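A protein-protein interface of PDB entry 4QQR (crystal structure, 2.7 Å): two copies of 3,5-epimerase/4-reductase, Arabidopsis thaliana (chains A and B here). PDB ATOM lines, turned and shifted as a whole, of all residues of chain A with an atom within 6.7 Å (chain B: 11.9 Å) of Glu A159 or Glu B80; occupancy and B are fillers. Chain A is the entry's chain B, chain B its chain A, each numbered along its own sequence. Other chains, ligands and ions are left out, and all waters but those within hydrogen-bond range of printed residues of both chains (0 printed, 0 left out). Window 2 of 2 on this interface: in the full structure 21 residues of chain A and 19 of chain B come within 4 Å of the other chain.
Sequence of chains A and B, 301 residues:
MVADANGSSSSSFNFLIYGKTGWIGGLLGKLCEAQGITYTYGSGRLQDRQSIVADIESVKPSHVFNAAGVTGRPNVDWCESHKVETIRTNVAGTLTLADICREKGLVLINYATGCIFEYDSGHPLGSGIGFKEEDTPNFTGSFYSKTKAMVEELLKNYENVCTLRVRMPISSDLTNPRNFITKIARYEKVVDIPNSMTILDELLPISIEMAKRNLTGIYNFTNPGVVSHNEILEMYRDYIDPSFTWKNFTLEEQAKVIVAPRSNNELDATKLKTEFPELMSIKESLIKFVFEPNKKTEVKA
No position is printed for both chains.
Of the 9 pairs that touch across the chains among the printed residues, none has its exchanged pair printed and touching as well.
Among the printed residues, pairs that only touch across the chains: Tyr A158 with Ile B87, Asn A157 with Phe B143, Asn A157 with Val B84, Arg A102 with Ser B81, Asn A157 with Ile B87, Glu A159 with Glu B80, Asn A157 with Glu B80 and Tyr A158 with Val B84.
Of chain B, only Glu B80 comes within 4 Å of Glu A159.
Glu B80 touches two residues of chain A.
Arg A102 touches one residue of chain B.
Of chain B, only Glu B80, Lys B83, Val B84, Ile B87 and Phe B143 come within 4 Å of Asn A157.
Of chain B, only Val B84 and Ile B87 come within 4 Å of Tyr A158.
No residue of chain B comes within 4 Å of Asn A160.
No residue of chain B comes within 4 Å of Val A161.
No residue of chain B comes within 4 Å of Thr A216.
Gly A217 touches none of the printed residues of chain B.
Printed residues of chain A within 4 Å of Ile B87: Asn A157 and Tyr A158.
Of the printed residues of chain A, Ser B81 touches Arg A102 (3.6 Å).
Of the printed residues of chain A, Lys B83 touches Asn A157.
Printed residues of chain A within 4 Å of Val B84: Asn A157 (3.5 Å) and Tyr A158 (3.9 Å).
Trp B78 touches none of the printed residues of chain A.
The nearest residue of chain B that does not touch Glu A159 is Val B84 (6.5 Å).
SG of Cys B79 lies close to N of Ser B81 (3.4 Å).
OG1 of Thr B147 is in hydrogen-bond range of O of Phe B143 (2.8 Å).
OG1 of Thr A216 sits close to O of Glu A159 (3.2 Å).
The side-chain amino group (NZ) of Lys B83 lies close to the side-chain amide oxygen (OD1) of Asn A157, 3.5 Å away.
Of the 18 printed residues of chain B, 6 touch a printed residue of chain A.
Printed residues of chain B that touch a printed residue of chain A: Glu B80, Ser B81, Lys B83, Val B84, Ile B87 and Phe B143.
Hydrophobic or aromatic side chains of chain B within 4 Å of the printed part of chain A: Val B84, Ile B87 and Phe B143.
Of the 13 printed residues of chain A, 4 touch a printed residue of chain B.
Printed residues of chain A that touch a printed residue of chain B: Arg A102, Asn A157, Tyr A158 and Glu A159.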
ATOM      1  N   ARG A 102      38.044 -18.831 -10.917  1.00  0.00           N
ATOM      2  CA  ARG A 102      37.758 -17.615 -11.666  1.00  0.00           C
ATOM      3  C   ARG A 102      38.042 -16.380 -10.820  1.00  0.00           C
ATOM      4  O   ARG A 102      38.683 -15.438 -11.290  1.00  0.00           O
ATOM      5  CB  ARG A 102      36.311 -17.608 -12.153  1.00  0.00           C
ATOM      6  CG  ARG A 102      35.956 -16.395 -12.990  1.00  0.00           C
ATOM      7  CD  ARG A 102      34.500 -16.423 -13.401  1.00  0.00           C
ATOM      8  NE  ARG A 102      34.141 -15.237 -14.164  1.00  0.00           N
ATOM      9  CZ  ARG A 102      33.739 -14.102 -13.600  1.00  0.00           C
ATOM     10  NH1 ARG A 102      33.652 -14.020 -12.273  1.00  0.00           N
ATOM     11  NH2 ARG A 102      33.417 -13.054 -14.356  1.00  0.00           N
ATOM     12  N   LEU A 155      29.179 -23.925 -17.510  1.00  0.00           N
ATOM     13  CA  LEU A 155      30.610 -23.601 -17.450  1.00  0.00           C
ATOM     14  C   LEU A 155      31.073 -22.611 -18.527  1.00  0.00           C
ATOM     15  O   LEU A 155      32.180 -22.068 -18.451  1.00  0.00           O
ATOM     16  CB  LEU A 155      31.475 -24.865 -17.503  1.00  0.00           C
ATOM     17  CG  LEU A 155      31.635 -25.635 -16.190  1.00  0.00           C
ATOM     18  CD1 LEU A 155      32.654 -26.742 -16.335  1.00  0.00           C
ATOM     19  CD2 LEU A 155      32.019 -24.677 -15.066  1.00  0.00           C
ATOM     20  N   LYS A 156      30.221 -22.392 -19.526  1.00  0.00           N
ATOM     21  CA  LYS A 156      30.513 -21.489 -20.632  1.00  0.00           C
ATOM     22  C   LYS A 156      30.694 -20.061 -20.124  1.00  0.00           C
ATOM     23  O   LYS A 156      31.443 -19.266 -20.715  1.00  0.00           O
ATOM     24  CB  LYS A 156      29.356 -21.505 -21.639  1.00  0.00           C
ATOM     25  CG  LYS A 156      29.262 -22.713 -22.562  1.00  0.00           C
ATOM     26  CD  LYS A 156      28.036 -22.533 -23.449  1.00  0.00           C
ATOM     27  CE  LYS A 156      27.948 -23.521 -24.602  1.00  0.00           C
ATOM     28  NZ  LYS A 156      26.640 -23.356 -25.333  1.00  0.00           N
ATOM     29  N   ASN A 157      29.993 -19.743 -19.035  1.00  0.00           N
ATOM     30  CA  ASN A 157      30.019 -18.393 -18.469  1.00  0.00           C
ATOM     31  C   ASN A 157      31.277 -18.101 -17.652  1.00  0.00           C
ATOM     32  O   ASN A 157      31.409 -17.026 -17.059  1.00  0.00           O
ATOM     33  CB  ASN A 157      28.779 -18.153 -17.617  1.00  0.00           C
ATOM     34  CG  ASN A 157      27.489 -18.404 -18.380  1.00  0.00           C
ATOM     35  OD1 ASN A 157      27.237 -17.811 -19.434  1.00  0.00           O
ATOM     36  ND2 ASN A 157      26.676 -19.307 -17.861  1.00  0.00           N
ATOM     37  N   TYR A 158      32.203 -19.060 -17.640  1.00  0.00           N
ATOM     38  CA  TYR A 158      33.429 -18.953 -16.862  1.00  0.00           C
ATOM     39  C   TYR A 158      34.626 -18.853 -17.795  1.00  0.00           C
ATOM     40  O   TYR A 158      35.223 -19.869 -18.173  1.00  0.00           O
ATOM     41  CB  TYR A 158      33.586 -20.163 -15.937  1.00  0.00           C
ATOM     42  CG  TYR A 158      32.520 -20.294 -14.872  1.00  0.00           C
ATOM     43  CD1 TYR A 158      32.813 -20.031 -13.535  1.00  0.00           C
ATOM     44  CD2 TYR A 158      31.225 -20.702 -15.192  1.00  0.00           C
ATOM     45  CE1 TYR A 158      31.847 -20.155 -12.552  1.00  0.00           C
ATOM     46  CE2 TYR A 158      30.258 -20.830 -14.207  1.00  0.00           C
ATOM     47  CZ  TYR A 158      30.580 -20.554 -12.895  1.00  0.00           C
ATOM     48  OH  TYR A 158      29.629 -20.679 -11.918  1.00  0.00           O
ATOM     49  N   GLU A 159      34.978 -17.623 -18.149  1.00  0.00           N
ATOM     50  CA  GLU A 159      36.034 -17.348 -19.126  1.00  0.00           C
ATOM     51  C   GLU A 159      37.341 -18.119 -18.908  1.00  0.00           C
ATOM     52  O   GLU A 159      38.088 -18.341 -19.853  1.00  0.00           O
ATOM     53  CB  GLU A 159      36.341 -15.854 -19.138  1.00  0.00           C
ATOM     54  CG  GLU A 159      36.887 -15.368 -17.800  1.00  0.00           C
ATOM     55  CD  GLU A 159      37.175 -13.894 -17.794  1.00  0.00           C
ATOM     56  OE1 GLU A 159      37.511 -13.350 -18.873  1.00  0.00           O
ATOM     57  OE2 GLU A 159      37.054 -13.280 -16.713  1.00  0.00           O
ATOM     58  N   ASN A 160      37.618 -18.511 -17.669  1.00  0.00           N
ATOM     59  CA  ASN A 160      38.870 -19.183 -17.333  1.00  0.00           C
ATOM     60  C   ASN A 160      38.811 -20.692 -17.542  1.00  0.00           C
ATOM     61  O   ASN A 160      39.843 -21.343 -17.684  1.00  0.00           O
ATOM     62  CB  ASN A 160      39.208 -18.942 -15.872  1.00  0.00           C
ATOM     63  CG  ASN A 160      38.230 -19.638 -14.934  1.00  0.00           C
ATOM     64  OD1 ASN A 160      37.014 -19.411 -15.012  1.00  0.00           O
ATOM     65  ND2 ASN A 160      38.753 -20.499 -14.054  1.00  0.00           N
ATOM     66  N   VAL A 161      37.607 -21.253 -17.527  1.00  0.00           N
ATOM     67  CA  VAL A 161      37.479 -22.687 -17.661  1.00  0.00           C
ATOM     68  C   VAL A 161      37.672 -23.170 -19.097  1.00  0.00           C
ATOM     69  O   VAL A 161      37.144 -22.586 -20.051  1.00  0.00           O
ATOM     70  CB  VAL A 161      36.140 -23.190 -17.103  1.00  0.00           C
ATOM     71  CG1 VAL A 161      35.945 -24.668 -17.424  1.00  0.00           C
ATOM     72  CG2 VAL A 161      36.068 -22.935 -15.599  1.00  0.00           C
ATOM     73  N   CYS A 162      38.463 -24.235 -19.225  1.00  0.00           N
ATOM     74  CA  CYS A 162      38.621 -24.988 -20.461  1.00  0.00           C
ATOM     75  C   CYS A 162      38.009 -26.378 -20.262  1.00  0.00           C
ATOM     76  O   CYS A 162      38.470 -27.159 -19.429  1.00  0.00           O
ATOM     77  CB  CYS A 162      40.109 -25.119 -20.800  1.00  0.00           C
ATOM     78  SG  CYS A 162      40.445 -25.819 -22.434  1.00  0.00           S
ATOM     79  N   ASN A 214      47.082 -21.313 -21.917  1.00  0.00           N
ATOM     80  CA  ASN A 214      45.885 -20.662 -21.383  1.00  0.00           C
ATOM     81  C   ASN A 214      44.674 -20.736 -22.309  1.00  0.00           C
ATOM     82  O   ASN A 214      43.937 -19.751 -22.476  1.00  0.00           O
ATOM     83  CB  ASN A 214      46.151 -19.195 -21.034  1.00  0.00           C
ATOM     84  CG  ASN A 214      47.252 -19.025 -20.030  1.00  0.00           C
ATOM     85  OD1 ASN A 214      47.365 -19.786 -19.065  1.00  0.00           O
ATOM     86  ND2 ASN A 214      48.091 -18.020 -20.254  1.00  0.00           N
ATOM     87  N   LEU A 215      44.464 -21.901 -22.906  1.00  0.00           N
ATOM     88  CA  LEU A 215      43.298 -22.095 -23.752  1.00  0.00           C
ATOM     89  C   LEU A 215      42.073 -22.278 -22.874  1.00  0.00           C
ATOM     90  O   LEU A 215      42.157 -22.861 -21.797  1.00  0.00           O
ATOM     91  CB  LEU A 215      43.492 -23.283 -24.689  1.00  0.00           C
ATOM     92  CG  LEU A 215      44.839 -23.258 -25.414  1.00  0.00           C
ATOM     93  CD1 LEU A 215      44.977 -24.491 -26.282  1.00  0.00           C
ATOM     94  CD2 LEU A 215      45.022 -21.977 -26.241  1.00  0.00           C
ATOM     95  N   THR A 216      40.952 -21.725 -23.329  1.00  0.00           N
ATOM     96  CA  THR A 216      39.694 -21.748 -22.599  1.00  0.00           C
ATOM     97  C   THR A 216      38.544 -21.923 -23.602  1.00  0.00           C
ATOM     98  O   THR A 216      38.759 -21.824 -24.815  1.00  0.00           O
ATOM     99  CB  THR A 216      39.484 -20.438 -21.781  1.00  0.00           C
ATOM    100  OG1 THR A 216      39.206 -19.346 -22.669  1.00  0.00           O
ATOM    101  CG2 THR A 216      40.709 -20.109 -20.895  1.00  0.00           C
ATOM    102  N   GLY A 217      37.332 -22.171 -23.097  1.00  0.00           N
ATOM    103  CA  GLY A 217      36.196 -22.529 -23.938  1.00  0.00           C
ATOM    104  C   GLY A 217      36.029 -24.041 -23.947  1.00  0.00           C
ATOM    105  O   GLY A 217      36.591 -24.735 -23.101  1.00  0.00           O
ATOM    106  N   VAL B  76      18.664  -7.555 -13.684  1.00  0.00           N
ATOM    107  CA  VAL B  76      19.837  -6.757 -14.007  1.00  0.00           C
ATOM    108  C   VAL B  76      20.386  -7.241 -15.340  1.00  0.00           C
ATOM    109  O   VAL B  76      19.728  -8.010 -16.038  1.00  0.00           O
ATOM    110  CB  VAL B  76      20.930  -6.892 -12.934  1.00  0.00           C
ATOM    111  CG1 VAL B  76      21.098  -5.583 -12.178  1.00  0.00           C
ATOM    112  CG2 VAL B  76      20.602  -8.031 -11.982  1.00  0.00           C
ATOM    113  N   ASP B  77      21.588  -6.803 -15.696  1.00  0.00           N
ATOM    114  CA  ASP B  77      22.204  -7.273 -16.928  1.00  0.00           C
ATOM    115  C   ASP B  77      22.701  -8.700 -16.762  1.00  0.00           C
ATOM    116  O   ASP B  77      22.994  -9.139 -15.650  1.00  0.00           O
ATOM    117  CB  ASP B  77      23.370  -6.366 -17.324  1.00  0.00           C
ATOM    118  CG  ASP B  77      24.414  -6.254 -16.232  1.00  0.00           C
ATOM    119  OD1 ASP B  77      24.327  -5.302 -15.429  1.00  0.00           O
ATOM    120  OD2 ASP B  77      25.319  -7.114 -16.173  1.00  0.00           O
ATOM    121  N   TRP B  78      22.798  -9.424 -17.870  1.00  0.00           N
ATOM    122  CA  TRP B  78      23.354 -10.772 -17.842  1.00  0.00           C
ATOM    123  C   TRP B  78      24.777 -10.901 -18.386  1.00  0.00           C
ATOM    124  O   TRP B  78      25.057 -11.671 -19.304  1.00  0.00           O
ATOM    125  CB  TRP B  78      22.385 -11.748 -18.508  1.00  0.00           C
ATOM    126  CG  TRP B  78      21.125 -11.882 -17.719  1.00  0.00           C
ATOM    127  CD1 TRP B  78      19.863 -11.519 -18.106  1.00  0.00           C
ATOM    128  CD2 TRP B  78      21.004 -12.389 -16.386  1.00  0.00           C
ATOM    129  NE1 TRP B  78      18.958 -11.789 -17.099  1.00  0.00           N
ATOM    130  CE2 TRP B  78      19.635 -12.321 -16.032  1.00  0.00           C
ATOM    131  CE3 TRP B  78      21.919 -12.898 -15.457  1.00  0.00           C
ATOM    132  CZ2 TRP B  78      19.164 -12.744 -14.788  1.00  0.00           C
ATOM    133  CZ3 TRP B  78      21.453 -13.314 -14.224  1.00  0.00           C
ATOM    134  CH2 TRP B  78      20.084 -13.238 -13.900  1.00  0.00           C
ATOM    135  N   CYS B  79      25.685 -10.141 -17.795  1.00  0.00           N
ATOM    136  CA  CYS B  79      27.087 -10.327 -18.093  1.00  0.00           C
ATOM    137  C   CYS B  79      27.628 -11.546 -17.327  1.00  0.00           C
ATOM    138  O   CYS B  79      26.924 -12.178 -16.522  1.00  0.00           O
ATOM    139  CB  CYS B  79      27.888  -9.083 -17.737  1.00  0.00           C
ATOM    140  SG  CYS B  79      28.430  -9.042 -16.010  1.00  0.00           S
ATOM    141  N   GLU B  80      28.886 -11.865 -17.584  1.00  0.00           N
ATOM    142  CA  GLU B  80      29.496 -13.008 -16.939  1.00  0.00           C
ATOM    143  C   GLU B  80      29.467 -12.927 -15.416  1.00  0.00           C
ATOM    144  O   GLU B  80      28.980 -13.857 -14.768  1.00  0.00           O
ATOM    145  CB  GLU B  80      30.897 -13.245 -17.492  1.00  0.00           C
ATOM    146  CG  GLU B  80      30.832 -13.620 -18.953  1.00  0.00           C
ATOM    147  CD  GLU B  80      32.190 -13.770 -19.581  1.00  0.00           C
ATOM    148  OE1 GLU B  80      33.197 -13.686 -18.837  1.00  0.00           O
ATOM    149  OE2 GLU B  80      32.245 -13.966 -20.814  1.00  0.00           O
ATOM    150  N   SER B  81      29.938 -11.817 -14.851  1.00  0.00           N
ATOM    151  CA  SER B  81      29.928 -11.650 -13.392  1.00  0.00           C
ATOM    152  C   SER B  81      28.525 -11.831 -12.800  1.00  0.00           C
ATOM    153  O   SER B  81      28.381 -12.308 -11.677  1.00  0.00           O
ATOM    154  CB  SER B  81      30.497 -10.294 -12.961  1.00  0.00           C
ATOM    155  OG  SER B  81      31.682  -9.953 -13.663  1.00  0.00           O
ATOM    156  N   HIS B  82      27.496 -11.466 -13.556  1.00  0.00           N
ATOM    157  CA  HIS B  82      26.139 -11.553 -13.048  1.00  0.00           C
ATOM    158  C   HIS B  82      25.569 -12.949 -13.216  1.00  0.00           C
ATOM    159  O   HIS B  82      24.877 -13.453 -12.331  1.00  0.00           O
ATOM    160  CB  HIS B  82      25.240 -10.520 -13.725  1.00  0.00           C
ATOM    161  CG  HIS B  82      24.895  -9.359 -12.850  1.00  0.00           C
ATOM    162  ND1 HIS B  82      24.923  -8.057 -13.293  1.00  0.00           N
ATOM    163  CD2 HIS B  82      24.514  -9.303 -11.552  1.00  0.00           C
ATOM    164  CE1 HIS B  82      24.576  -7.246 -12.310  1.00  0.00           C
ATOM    165  NE2 HIS B  82      24.317  -7.978 -11.242  1.00  0.00           N
ATOM    166  N   LYS B  83      25.850 -13.561 -14.363  1.00  0.00           N
ATOM    167  CA  LYS B  83      25.450 -14.938 -14.600  1.00  0.00           C
ATOM    168  C   LYS B  83      26.115 -15.842 -13.563  1.00  0.00           C
ATOM    169  O   LYS B  83      25.449 -16.692 -12.953  1.00  0.00           O
ATOM    170  CB  LYS B  83      25.847 -15.385 -16.012  1.00  0.00           C
ATOM    171  CG  LYS B  83      24.991 -14.843 -17.144  1.00  0.00           C
ATOM    172  CD  LYS B  83      25.688 -15.146 -18.454  1.00  0.00           C
ATOM    173  CE  LYS B  83      24.753 -15.083 -19.654  1.00  0.00           C
ATOM    174  NZ  LYS B  83      25.571 -15.124 -20.918  1.00  0.00           N
ATOM    175  N   VAL B  84      27.423 -15.652 -13.367  1.00  0.00           N
ATOM    176  CA  VAL B  84      28.185 -16.490 -12.443  1.00  0.00           C
ATOM    177  C   VAL B  84      27.614 -16.330 -11.051  1.00  0.00           C
ATOM    178  O   VAL B  84      27.457 -17.306 -10.318  1.00  0.00           O
ATOM    179  CB  VAL B  84      29.714 -16.175 -12.449  1.00  0.00           C
ATOM    180  CG1 VAL B  84      30.396 -16.750 -11.221  1.00  0.00           C
ATOM    181  CG2 VAL B  84      30.372 -16.722 -13.711  1.00  0.00           C
ATOM    182  N   GLU B  85      27.259 -15.097 -10.709  1.00  0.00           N
ATOM    183  CA  GLU B  85      26.717 -14.801  -9.396  1.00  0.00           C
ATOM    184  C   GLU B  85      25.428 -15.583  -9.132  1.00  0.00           C
ATOM    185  O   GLU B  85      25.200 -16.028  -8.022  1.00  0.00           O
ATOM    186  CB  GLU B  85      26.522 -13.293  -9.203  1.00  0.00           C
ATOM    187  N   THR B  86      24.601 -15.785 -10.149  1.00  0.00           N
ATOM    188  CA  THR B  86      23.368 -16.540  -9.929  1.00  0.00           C
ATOM    189  C   THR B  86      23.643 -18.048  -9.884  1.00  0.00           C
ATOM    190  O   THR B  86      22.908 -18.814  -9.257  1.00  0.00           O
ATOM    191  CB  THR B  86      22.300 -16.235 -10.989  1.00  0.00           C
ATOM    192  OG1 THR B  86      22.476 -14.903 -11.477  1.00  0.00           O
ATOM    193  CG2 THR B  86      20.904 -16.360 -10.380  1.00  0.00           C
ATOM    194  N   ILE B  87      24.704 -18.470 -10.561  1.00  0.00           N
ATOM    195  CA  ILE B  87      25.066 -19.879 -10.587  1.00  0.00           C
ATOM    196  C   ILE B  87      25.591 -20.319  -9.228  1.00  0.00           C
ATOM    197  O   ILE B  87      25.332 -21.435  -8.782  1.00  0.00           O
ATOM    198  CB  ILE B  87      26.132 -20.172 -11.659  1.00  0.00           C
ATOM    199  CG1 ILE B  87      25.521 -20.077 -13.058  1.00  0.00           C
ATOM    200  CG2 ILE B  87      26.743 -21.545 -11.438  1.00  0.00           C
ATOM    201  CD1 ILE B  87      26.531 -20.213 -14.174  1.00  0.00           C
ATOM    202  N   ARG B  88      26.327 -19.429  -8.571  1.00  0.00           N
ATOM    203  CA  ARG B  88      26.915 -19.729  -7.272  1.00  0.00           C
ATOM    204  C   ARG B  88      25.855 -19.867  -6.185  1.00  0.00           C
ATOM    205  O   ARG B  88      25.953 -20.735  -5.320  1.00  0.00           O
ATOM    206  CB  ARG B  88      27.929 -18.652  -6.885  1.00  0.00           C
ATOM    207  CG  ARG B  88      28.529 -18.833  -5.501  1.00  0.00           C
ATOM    208  CD  ARG B  88      29.055 -17.517  -4.958  1.00  0.00           C
ATOM    209  NE  ARG B  88      29.085 -16.481  -5.986  1.00  0.00           N
ATOM    210  CZ  ARG B  88      30.087 -15.625  -6.155  1.00  0.00           C
ATOM    211  NH1 ARG B  88      31.148 -15.679  -5.361  1.00  0.00           N
ATOM    212  NH2 ARG B  88      30.030 -14.716  -7.118  1.00  0.00           N
ATOM    213  N   THR B  89      24.843 -19.007  -6.232  1.00  0.00           N
ATOM    214  CA  THR B  89      23.796 -19.028  -5.234  1.00  0.00           C
ATOM    215  C   THR B  89      22.563 -19.846  -5.622  1.00  0.00           C
ATOM    216  O   THR B  89      22.033 -20.574  -4.787  1.00  0.00           O
ATOM    217  CB  THR B  89      23.412 -17.600  -4.729  1.00  0.00           C
ATOM    218  OG1 THR B  89      22.090 -17.624  -4.169  1.00  0.00           O
ATOM    219  CG2 THR B  89      23.416 -16.613  -5.833  1.00  0.00           C
ATOM    220  N   VAL B  91      22.249 -22.113  -8.231  1.00  0.00           N
ATOM    221  CA  VAL B  91      22.605 -23.462  -8.595  1.00  0.00           C
ATOM    222  C   VAL B  91      23.389 -24.124  -7.455  1.00  0.00           C
ATOM    223  O   VAL B  91      22.826 -24.915  -6.698  1.00  0.00           O
ATOM    224  CB  VAL B  91      23.375 -23.519  -9.940  1.00  0.00           C
ATOM    225  CG1 VAL B  91      23.672 -24.939 -10.313  1.00  0.00           C
ATOM    226  CG2 VAL B  91      22.553 -22.893 -11.044  1.00  0.00           C
ATOM    227  N   PHE B 143      19.173 -16.904 -20.275  1.00  0.00           N
ATOM    228  CA  PHE B 143      20.013 -17.515 -19.238  1.00  0.00           C
ATOM    229  C   PHE B 143      19.273 -17.817 -17.934  1.00  0.00           C
ATOM    230  O   PHE B 143      19.312 -18.942 -17.428  1.00  0.00           O
ATOM    231  CB  PHE B 143      21.219 -16.630 -18.930  1.00  0.00           C
ATOM    232  CG  PHE B 143      21.947 -17.022 -17.676  1.00  0.00           C
ATOM    233  CD1 PHE B 143      22.883 -18.059 -17.695  1.00  0.00           C
ATOM    234  CD2 PHE B 143      21.692 -16.360 -16.464  1.00  0.00           C
ATOM    235  CE1 PHE B 143      23.553 -18.427 -16.542  1.00  0.00           C
ATOM    236  CE2 PHE B 143      22.362 -16.718 -15.306  1.00  0.00           C
ATOM    237  CZ  PHE B 143      23.301 -17.755 -15.344  1.00  0.00           C
ATOM    238  N   TYR B 144      18.622 -16.803 -17.386  1.00  0.00           N
ATOM    239  CA  TYR B 144      17.905 -16.978 -16.139  1.00  0.00           C
ATOM    240  C   TYR B 144      16.934 -18.150 -16.256  1.00  0.00           C
ATOM    241  O   TYR B 144      16.892 -19.028 -15.399  1.00  0.00           O
ATOM    242  CB  TYR B 144      17.167 -15.690 -15.730  1.00  0.00           C
ATOM    243  CG  TYR B 144      16.648 -15.783 -14.320  1.00  0.00           C
ATOM    244  CD1 TYR B 144      17.524 -15.746 -13.249  1.00  0.00           C
ATOM    245  CD2 TYR B 144      15.295 -15.958 -14.061  1.00  0.00           C
ATOM    246  CE1 TYR B 144      17.071 -15.860 -11.960  1.00  0.00           C
ATOM    247  CE2 TYR B 144      14.825 -16.075 -12.772  1.00  0.00           C
ATOM    248  CZ  TYR B 144      15.721 -16.030 -11.720  1.00  0.00           C
ATOM    249  OH  TYR B 144      15.288 -16.140 -10.414  1.00  0.00           O
ATOM    250  N   THR B 147      18.589 -21.607 -16.580  1.00  0.00           N
ATOM    251  CA  THR B 147      19.229 -21.934 -15.313  1.00  0.00           C
ATOM    252  C   THR B 147      18.234 -22.416 -14.254  1.00  0.00           C
ATOM    253  O   THR B 147      18.460 -23.449 -13.595  1.00  0.00           O
ATOM    254  CB  THR B 147      20.055 -20.753 -14.785  1.00  0.00           C
ATOM    255  OG1 THR B 147      21.049 -20.402 -15.757  1.00  0.00           O
ATOM    256  CG2 THR B 147      20.745 -21.119 -13.498  1.00  0.00           C
